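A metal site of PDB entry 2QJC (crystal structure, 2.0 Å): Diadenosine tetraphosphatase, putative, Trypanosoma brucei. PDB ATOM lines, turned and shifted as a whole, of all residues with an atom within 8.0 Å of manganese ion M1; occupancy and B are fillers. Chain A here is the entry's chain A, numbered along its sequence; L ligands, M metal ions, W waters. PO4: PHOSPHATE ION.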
ATOM      1  N   ASP A  26      -1.436  20.419  -1.575  1.00  0.00           N
ATOM      2  CA  ASP A  26      -2.651  20.789  -2.308  1.00  0.00           C
ATOM      3  C   ASP A  26      -3.506  21.811  -1.556  1.00  0.00           C
ATOM      4  O   ASP A  26      -3.993  21.542  -0.466  1.00  0.00           O
ATOM      5  CB  ASP A  26      -3.484  19.522  -2.613  1.00  0.00           C
ATOM      6  CG  ASP A  26      -2.743  18.521  -3.509  1.00  0.00           C
ATOM      7  OD1 ASP A  26      -1.553  18.240  -3.241  1.00  0.00           O
ATOM      8  OD2 ASP A  26      -3.360  18.007  -4.473  1.00  0.00           O
ATOM      9  N   HIS A  28      -6.286  23.679  -3.163  1.00  0.00           N
ATOM     10  CA  HIS A  28      -7.673  23.547  -3.583  1.00  0.00           C
ATOM     11  C   HIS A  28      -8.601  24.650  -3.069  1.00  0.00           C
ATOM     12  O   HIS A  28      -9.569  24.381  -2.356  1.00  0.00           O
ATOM     13  CB  HIS A  28      -8.231  22.172  -3.150  1.00  0.00           C
ATOM     14  CG  HIS A  28      -7.877  21.061  -4.092  1.00  0.00           C
ATOM     15  ND1 HIS A  28      -8.224  21.069  -5.417  1.00  0.00           N
ATOM     16  CD2 HIS A  28      -7.229  19.889  -3.880  1.00  0.00           C
ATOM     17  CE1 HIS A  28      -7.809  19.950  -5.988  1.00  0.00           C
ATOM     18  NE2 HIS A  28      -7.200  19.211  -5.075  1.00  0.00           N
ATOM     19  N   VAL A  53       2.672  22.862  -4.763  1.00  0.00           N
ATOM     20  CA  VAL A  53       2.768  21.608  -5.502  1.00  0.00           C
ATOM     21  C   VAL A  53       1.656  21.511  -6.572  1.00  0.00           C
ATOM     22  O   VAL A  53       1.531  20.514  -7.280  1.00  0.00           O
ATOM     23  CB  VAL A  53       2.659  20.371  -4.578  1.00  0.00           C
ATOM     24  CG1 VAL A  53       3.789  20.403  -3.533  1.00  0.00           C
ATOM     25  CG2 VAL A  53       1.282  20.302  -3.925  1.00  0.00           C
ATOM     26  N   GLY A  54       0.855  22.566  -6.690  1.00  0.00           N
ATOM     27  CA  GLY A  54      -0.204  22.555  -7.688  1.00  0.00           C
ATOM     28  C   GLY A  54      -1.557  22.218  -7.102  1.00  0.00           C
ATOM     29  O   GLY A  54      -1.667  21.906  -5.916  1.00  0.00           O
ATOM     30  N   ASP A  55      -2.585  22.248  -7.943  1.00  0.00           N
ATOM     31  CA  ASP A  55      -3.955  21.969  -7.512  1.00  0.00           C
ATOM     32  C   ASP A  55      -4.340  23.130  -6.614  1.00  0.00           C
ATOM     33  O   ASP A  55      -4.725  22.961  -5.454  1.00  0.00           O
ATOM     34  CB  ASP A  55      -4.031  20.627  -6.753  1.00  0.00           C
ATOM     35  CG  ASP A  55      -4.526  19.489  -7.630  1.00  0.00           C
ATOM     36  OD1 ASP A  55      -4.470  19.628  -8.876  1.00  0.00           O
ATOM     37  OD2 ASP A  55      -4.955  18.451  -7.087  1.00  0.00           O
ATOM     38  N   LEU A  79       2.296  22.836 -12.023  1.00  0.00           N
ATOM     39  CA  LEU A  79       0.935  22.618 -12.492  1.00  0.00           C
ATOM     40  C   LEU A  79       0.333  21.324 -11.959  1.00  0.00           C
ATOM     41  O   LEU A  79       0.940  20.263 -12.085  1.00  0.00           O
ATOM     42  CB  LEU A  79       0.914  22.582 -14.022  1.00  0.00           C
ATOM     43  CG  LEU A  79      -0.443  22.547 -14.714  1.00  0.00           C
ATOM     44  CD1 LEU A  79      -1.257  23.778 -14.319  1.00  0.00           C
ATOM     45  CD2 LEU A  79      -0.236  22.504 -16.216  1.00  0.00           C
ATOM     46  N   GLY A  80      -0.845  21.430 -11.337  1.00  0.00           N
ATOM     47  CA  GLY A  80      -1.534  20.256 -10.810  1.00  0.00           C
ATOM     48  C   GLY A  80      -2.493  19.719 -11.862  1.00  0.00           C
ATOM     49  O   GLY A  80      -2.722  20.383 -12.867  1.00  0.00           O
ATOM     50  N   ASN A  81      -3.070  18.526 -11.660  1.00  0.00           N
ATOM     51  CA  ASN A  81      -3.970  18.028 -12.695  1.00  0.00           C
ATOM     52  C   ASN A  81      -5.330  18.705 -12.704  1.00  0.00           C
ATOM     53  O   ASN A  81      -6.016  18.684 -13.727  1.00  0.00           O
ATOM     54  CB  ASN A  81      -4.126  16.494 -12.634  1.00  0.00           C
ATOM     55  CG  ASN A  81      -4.736  16.030 -11.342  1.00  0.00           C
ATOM     56  OD1 ASN A  81      -5.697  15.249 -11.352  1.00  0.00           O
ATOM     57  ND2 ASN A  81      -4.184  16.483 -10.223  1.00  0.00           N
ATOM     58  N   HIS A  82      -5.728  19.300 -11.583  1.00  0.00           N
ATOM     59  CA  HIS A  82      -6.991  20.018 -11.548  1.00  0.00           C
ATOM     60  C   HIS A  82      -6.788  21.364 -12.213  1.00  0.00           C
ATOM     61  O   HIS A  82      -7.700  21.896 -12.858  1.00  0.00           O
ATOM     62  CB  HIS A  82      -7.471  20.200 -10.105  1.00  0.00           C
ATOM     63  CG  HIS A  82      -8.183  19.003  -9.563  1.00  0.00           C
ATOM     64  ND1 HIS A  82      -9.549  18.852  -9.656  1.00  0.00           N
ATOM     65  CD2 HIS A  82      -7.718  17.899  -8.927  1.00  0.00           C
ATOM     66  CE1 HIS A  82      -9.902  17.706  -9.100  1.00  0.00           C
ATOM     67  NE2 HIS A  82      -8.807  17.112  -8.653  1.00  0.00           N
ATOM     68  N   ASP A  83      -5.593  21.915 -12.068  1.00  0.00           N
ATOM     69  CA  ASP A  83      -5.274  23.184 -12.708  1.00  0.00           C
ATOM     70  C   ASP A  83      -5.277  22.923 -14.212  1.00  0.00           C
ATOM     71  O   ASP A  83      -5.838  23.697 -14.990  1.00  0.00           O
ATOM     72  CB  ASP A  83      -3.880  23.677 -12.310  1.00  0.00           C
ATOM     73  CG  ASP A  83      -3.734  23.883 -10.820  1.00  0.00           C
ATOM     74  OD1 ASP A  83      -4.661  24.434 -10.183  1.00  0.00           O
ATOM     75  OD2 ASP A  83      -2.660  23.512 -10.282  1.00  0.00           O
ATOM     76  N   LYS A  85      -6.769  20.478 -16.012  1.00  0.00           N
ATOM     77  CA  LYS A  85      -8.084  20.184 -16.573  1.00  0.00           C
ATOM     78  C   LYS A  85      -8.911  21.453 -16.709  1.00  0.00           C
ATOM     79  O   LYS A  85      -9.709  21.578 -17.645  1.00  0.00           O
ATOM     80  CB  LYS A  85      -8.841  19.170 -15.722  1.00  0.00           C
ATOM     81  CG  LYS A  85      -8.186  17.778 -15.656  1.00  0.00           C
ATOM     82  CD  LYS A  85      -9.054  16.789 -14.894  1.00  0.00           C
ATOM     83  CE  LYS A  85      -8.313  15.493 -14.617  1.00  0.00           C
ATOM     84  NZ  LYS A  85      -7.783  14.866 -15.865  1.00  0.00           N
ATOM     85  N   HIS A 141       3.920  17.699  -9.189  1.00  0.00           N
ATOM     86  CA  HIS A 141       2.602  17.551  -8.571  1.00  0.00           C
ATOM     87  C   HIS A 141       2.291  16.162  -7.995  1.00  0.00           C
ATOM     88  O   HIS A 141       1.861  16.062  -6.831  1.00  0.00           O
ATOM     89  CB  HIS A 141       1.485  17.957  -9.555  1.00  0.00           C
ATOM     90  CG  HIS A 141       0.107  17.771  -9.000  1.00  0.00           C
ATOM     91  ND1 HIS A 141      -0.353  18.481  -7.909  1.00  0.00           N
ATOM     92  CD2 HIS A 141      -0.871  16.900  -9.324  1.00  0.00           C
ATOM     93  CE1 HIS A 141      -1.565  18.057  -7.593  1.00  0.00           C
ATOM     94  NE2 HIS A 141      -1.905  17.094  -8.426  1.00  0.00           N
ATOM     95  N   ALA A 142       2.489  15.118  -8.792  1.00  0.00           N
ATOM     96  CA  ALA A 142       2.208  13.751  -8.333  1.00  0.00           C
ATOM     97  C   ALA A 142       3.471  12.924  -8.117  1.00  0.00           C
ATOM     98  O   ALA A 142       3.522  12.091  -7.202  1.00  0.00           O
ATOM     99  CB  ALA A 142       1.291  13.048  -9.349  1.00  0.00           C
ATOM    100  N   VAL A 158       3.651  12.904 -14.511  1.00  0.00           N
ATOM    101  CA  VAL A 158       4.036  13.823 -13.444  1.00  0.00           C
ATOM    102  C   VAL A 158       2.886  14.534 -12.737  1.00  0.00           C
ATOM    103  O   VAL A 158       3.055  15.083 -11.649  1.00  0.00           O
ATOM    104  CB  VAL A 158       5.058  14.883 -13.946  1.00  0.00           C
ATOM    105  CG1 VAL A 158       6.333  14.196 -14.422  1.00  0.00           C
ATOM    106  CG2 VAL A 158       4.436  15.705 -15.060  1.00  0.00           C
ATOM    107  N   THR A 159       1.692  14.524 -13.340  1.00  0.00           N
ATOM    108  CA  THR A 159       0.563  15.190 -12.713  1.00  0.00           C
ATOM    109  C   THR A 159      -0.526  14.258 -12.168  1.00  0.00           C
ATOM    110  O   THR A 159      -1.448  14.723 -11.497  1.00  0.00           O
ATOM    111  CB  THR A 159      -0.132  16.206 -13.669  1.00  0.00           C
ATOM    112  OG1 THR A 159      -0.542  15.530 -14.861  1.00  0.00           O
ATOM    113  CG2 THR A 159       0.821  17.332 -14.014  1.00  0.00           C
ATOM    114  N   THR A 160      -0.416  12.963 -12.453  1.00  0.00           N
ATOM    115  CA  THR A 160      -1.438  12.009 -11.996  1.00  0.00           C
ATOM    116  C   THR A 160      -0.994  10.686 -11.367  1.00  0.00           C
ATOM    117  O   THR A 160      -1.830   9.958 -10.828  1.00  0.00           O
ATOM    118  CB  THR A 160      -2.396  11.605 -13.153  1.00  0.00           C
ATOM    119  OG1 THR A 160      -1.706  10.745 -14.060  1.00  0.00           O
ATOM    120  CG2 THR A 160      -2.884  12.826 -13.916  1.00  0.00           C
ATOM    121  N   MET A 161       0.293  10.360 -11.420  1.00  0.00           N
ATOM    122  CA  MET A 161       0.745   9.064 -10.908  1.00  0.00           C
ATOM    123  C   MET A 161       0.601   8.795  -9.398  1.00  0.00           C
ATOM    124  O   MET A 161       0.877   9.660  -8.562  1.00  0.00           O
ATOM    125  CB  MET A 161       2.194   8.797 -11.324  1.00  0.00           C
ATOM    126  CG  MET A 161       3.262   9.467 -10.449  1.00  0.00           C
ATOM    127  SD  MET A 161       5.080   9.193 -11.118  1.00  0.00           S
ATOM    128  CE  MET A 161       5.270   7.303 -10.825  1.00  0.00           C
ATOM    129  N   ARG A 162       0.151   7.583  -9.079  1.00  0.00           N
ATOM    130  CA  ARG A 162      -0.002   7.146  -7.696  1.00  0.00           C
ATOM    131  C   ARG A 162       0.793   5.852  -7.496  1.00  0.00           C
ATOM    132  O   ARG A 162       1.416   5.632  -6.451  1.00  0.00           O
ATOM    133  CB  ARG A 162      -1.472   6.877  -7.369  1.00  0.00           C
ATOM    134  CG  ARG A 162      -2.360   8.100  -7.323  1.00  0.00           C
ATOM    135  CD  ARG A 162      -3.834   7.698  -7.245  1.00  0.00           C
ATOM    136  NE  ARG A 162      -4.729   8.753  -7.703  1.00  0.00           N
ATOM    137  CZ  ARG A 162      -5.125   9.777  -6.959  1.00  0.00           C
ATOM    138  NH1 ARG A 162      -4.696   9.895  -5.713  1.00  0.00           N
ATOM    139  NH2 ARG A 162      -5.952  10.692  -7.467  1.00  0.00           N
ATOM    140  N   GLU A 181      -2.264   6.244 -12.570  1.00  0.00           N
ATOM    141  CA  GLU A 181      -3.060   7.061 -11.660  1.00  0.00           C
ATOM    142  C   GLU A 181      -3.999   6.158 -10.865  1.00  0.00           C
ATOM    143  O   GLU A 181      -4.421   6.484  -9.758  1.00  0.00           O
ATOM    144  CB  GLU A 181      -3.870   8.074 -12.450  1.00  0.00           C
ATOM    145  CG  GLU A 181      -4.986   8.732 -11.684  1.00  0.00           C
ATOM    146  CD  GLU A 181      -5.745   9.733 -12.532  1.00  0.00           C
ATOM    147  OE1 GLU A 181      -5.905   9.461 -13.746  1.00  0.00           O
ATOM    148  OE2 GLU A 181      -6.193  10.769 -11.993  1.00  0.00           O
ATOM    149  N   GLY A 203       2.501  16.332  -3.915  1.00  0.00           N
ATOM    150  CA  GLY A 203       1.179  16.328  -3.282  1.00  0.00           C
ATOM    151  C   GLY A 203       0.285  15.344  -4.037  1.00  0.00           C
ATOM    152  O   GLY A 203       0.607  14.154  -4.100  1.00  0.00           O
ATOM    153  N   HIS A 204      -0.828  15.821  -4.568  1.00  0.00           N
ATOM    154  CA  HIS A 204      -1.767  15.007  -5.373  1.00  0.00           C
ATOM    155  C   HIS A 204      -2.537  13.834  -4.744  1.00  0.00           C
ATOM    156  O   HIS A 204      -3.771  13.794  -4.811  1.00  0.00           O
ATOM    157  CB  HIS A 204      -1.040  14.500  -6.620  1.00  0.00           C
ATOM    158  CG  HIS A 204      -1.873  13.593  -7.493  1.00  0.00           C
ATOM    159  ND1 HIS A 204      -3.043  14.010  -8.087  1.00  0.00           N
ATOM    160  CD2 HIS A 204      -1.681  12.324  -7.896  1.00  0.00           C
ATOM    161  CE1 HIS A 204      -3.542  13.024  -8.817  1.00  0.00           C
ATOM    162  NE2 HIS A 204      -2.728  11.985  -8.721  1.00  0.00           N
ATOM    163  N   ASP A 205      -1.810  12.876  -4.165  1.00  0.00           N
ATOM    164  CA  ASP A 205      -2.385  11.655  -3.595  1.00  0.00           C
ATOM    165  C   ASP A 205      -3.058  11.779  -2.220  1.00  0.00           C
ATOM    166  O   ASP A 205      -2.582  11.218  -1.235  1.00  0.00           O
ATOM    167  CB  ASP A 205      -1.280  10.573  -3.540  1.00  0.00           C
ATOM    168  CG  ASP A 205      -1.834   9.144  -3.433  1.00  0.00           C
ATOM    169  OD1 ASP A 205      -1.016   8.194  -3.420  1.00  0.00           O
ATOM    170  OD2 ASP A 205      -3.067   8.957  -3.354  1.00  0.00           O
ATOM    171  N   ALA A 206      -4.172  12.507  -2.165  1.00  0.00           N
ATOM    172  CA  ALA A 206      -4.912  12.710  -0.914  1.00  0.00           C
ATOM    173  C   ALA A 206      -5.320  11.388  -0.256  1.00  0.00           C
ATOM    174  O   ALA A 206      -5.402  11.299   0.967  1.00  0.00           O
ATOM    175  CB  ALA A 206      -6.170  13.561  -1.178  1.00  0.00           C
ATOM    176  N   ASP A 222       0.335  15.958   0.559  1.00  0.00           N
ATOM    177  CA  ASP A 222      -1.126  16.094   0.476  1.00  0.00           C
ATOM    178  C   ASP A 222      -1.869  15.496   1.674  1.00  0.00           C
ATOM    179  O   ASP A 222      -2.355  14.365   1.613  1.00  0.00           O
ATOM    180  CB  ASP A 222      -1.672  15.498  -0.820  1.00  0.00           C
ATOM    181  CG  ASP A 222      -3.104  15.947  -1.086  1.00  0.00           C
ATOM    182  OD1 ASP A 222      -3.694  16.604  -0.188  1.00  0.00           O
ATOM    183  OD2 ASP A 222      -3.637  15.652  -2.177  1.00  0.00           O
ATOM    184  N   TYR A 227     -10.481  18.407   2.249  1.00  0.00           N
ATOM    185  CA  TYR A 227     -11.394  17.351   2.688  1.00  0.00           C
ATOM    186  C   TYR A 227     -11.557  17.361   4.212  1.00  0.00           C
ATOM    187  O   TYR A 227     -12.137  16.426   4.779  1.00  0.00           O
ATOM    188  CB  TYR A 227     -10.866  15.988   2.254  1.00  0.00           C
ATOM    189  CG  TYR A 227     -10.674  15.820   0.765  1.00  0.00           C
ATOM    190  CD1 TYR A 227     -11.765  15.614  -0.091  1.00  0.00           C
ATOM    191  CD2 TYR A 227      -9.389  15.792   0.211  1.00  0.00           C
ATOM    192  CE1 TYR A 227     -11.580  15.379  -1.453  1.00  0.00           C
ATOM    193  CE2 TYR A 227      -9.192  15.568  -1.135  1.00  0.00           C
ATOM    194  CZ  TYR A 227     -10.276  15.354  -1.965  1.00  0.00           C
ATOM    195  OH  TYR A 227     -10.049  15.099  -3.299  1.00  0.00           O
HETATM  196  P   PO4 L   1      -6.959  14.680  -6.296  1.00  0.00           P
HETATM  197  O1  PO4 L   1      -7.416  14.829  -4.747  1.00  0.00           O
HETATM  198  O2  PO4 L   1      -6.169  13.313  -6.433  1.00  0.00           O
HETATM  199  O3  PO4 L   1      -8.234  14.677  -7.187  1.00  0.00           O
HETATM  200  O4  PO4 L   1      -6.010  15.870  -6.650  1.00  0.00           O
HETATM  201 MN    MN M   1      -4.007  16.086  -8.188  1.00  0.00          MN
HETATM  202 MN    MN M   2      -5.395  17.533  -5.247  1.00  0.00          MN
HETATM  203  O   HOH W   1      -6.594  14.553  -9.235  1.00  0.00           O
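The backbone NH (N) of Asp 55 lies within hydrogen-bond range of the side-chain carboxylate (OD2) of Asp 83 (2.7 Å). The backbone carbonyl oxygen (O) of His 141 is in hydrogen-bond range of the backbone NH (N) of Gly 203 (3.0 Å). OD1 of Asp 55 is in hydrogen-bond range of N of Asn 81, at 3.3 Å. A ring nitrogen (NE2) of His 204 lies within hydrogen-bond range of the backbone carbonyl oxygen of Thr 160. N of His 204 lies within hydrogen-bond range of OD1 of Asp 26 (2.9 Å). The side-chain amide nitrogen of Asn 81 sits close to the backbone carbonyl oxygen of Thr 159 (3.5 Å). N of His 82 lies within hydrogen-bond range of OD1 of Asp 55, 3.0 Å away. ND1 of His 141 lies within hydrogen-bond range of O of Val 53 (2.8 Å).
Manganese ion M1 is bound by ND2 of Asn 81 (2.1 Å). Manganese ion M1 is bound by ND1 of His 204, 2.3 Å away. Manganese ion M1 is bound by NE2 of His 141, 2.3 Å away. Manganese ion M1 is bound by an oxygen (O4) of the ligand. Slightly farther from manganese ion M1 lies OD2 of Asp 55 (2.8 Å).
Water W1 bridges OD1 of Asn 81 (2.4 Å) and NE2 of His 82 (3.4 Å).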
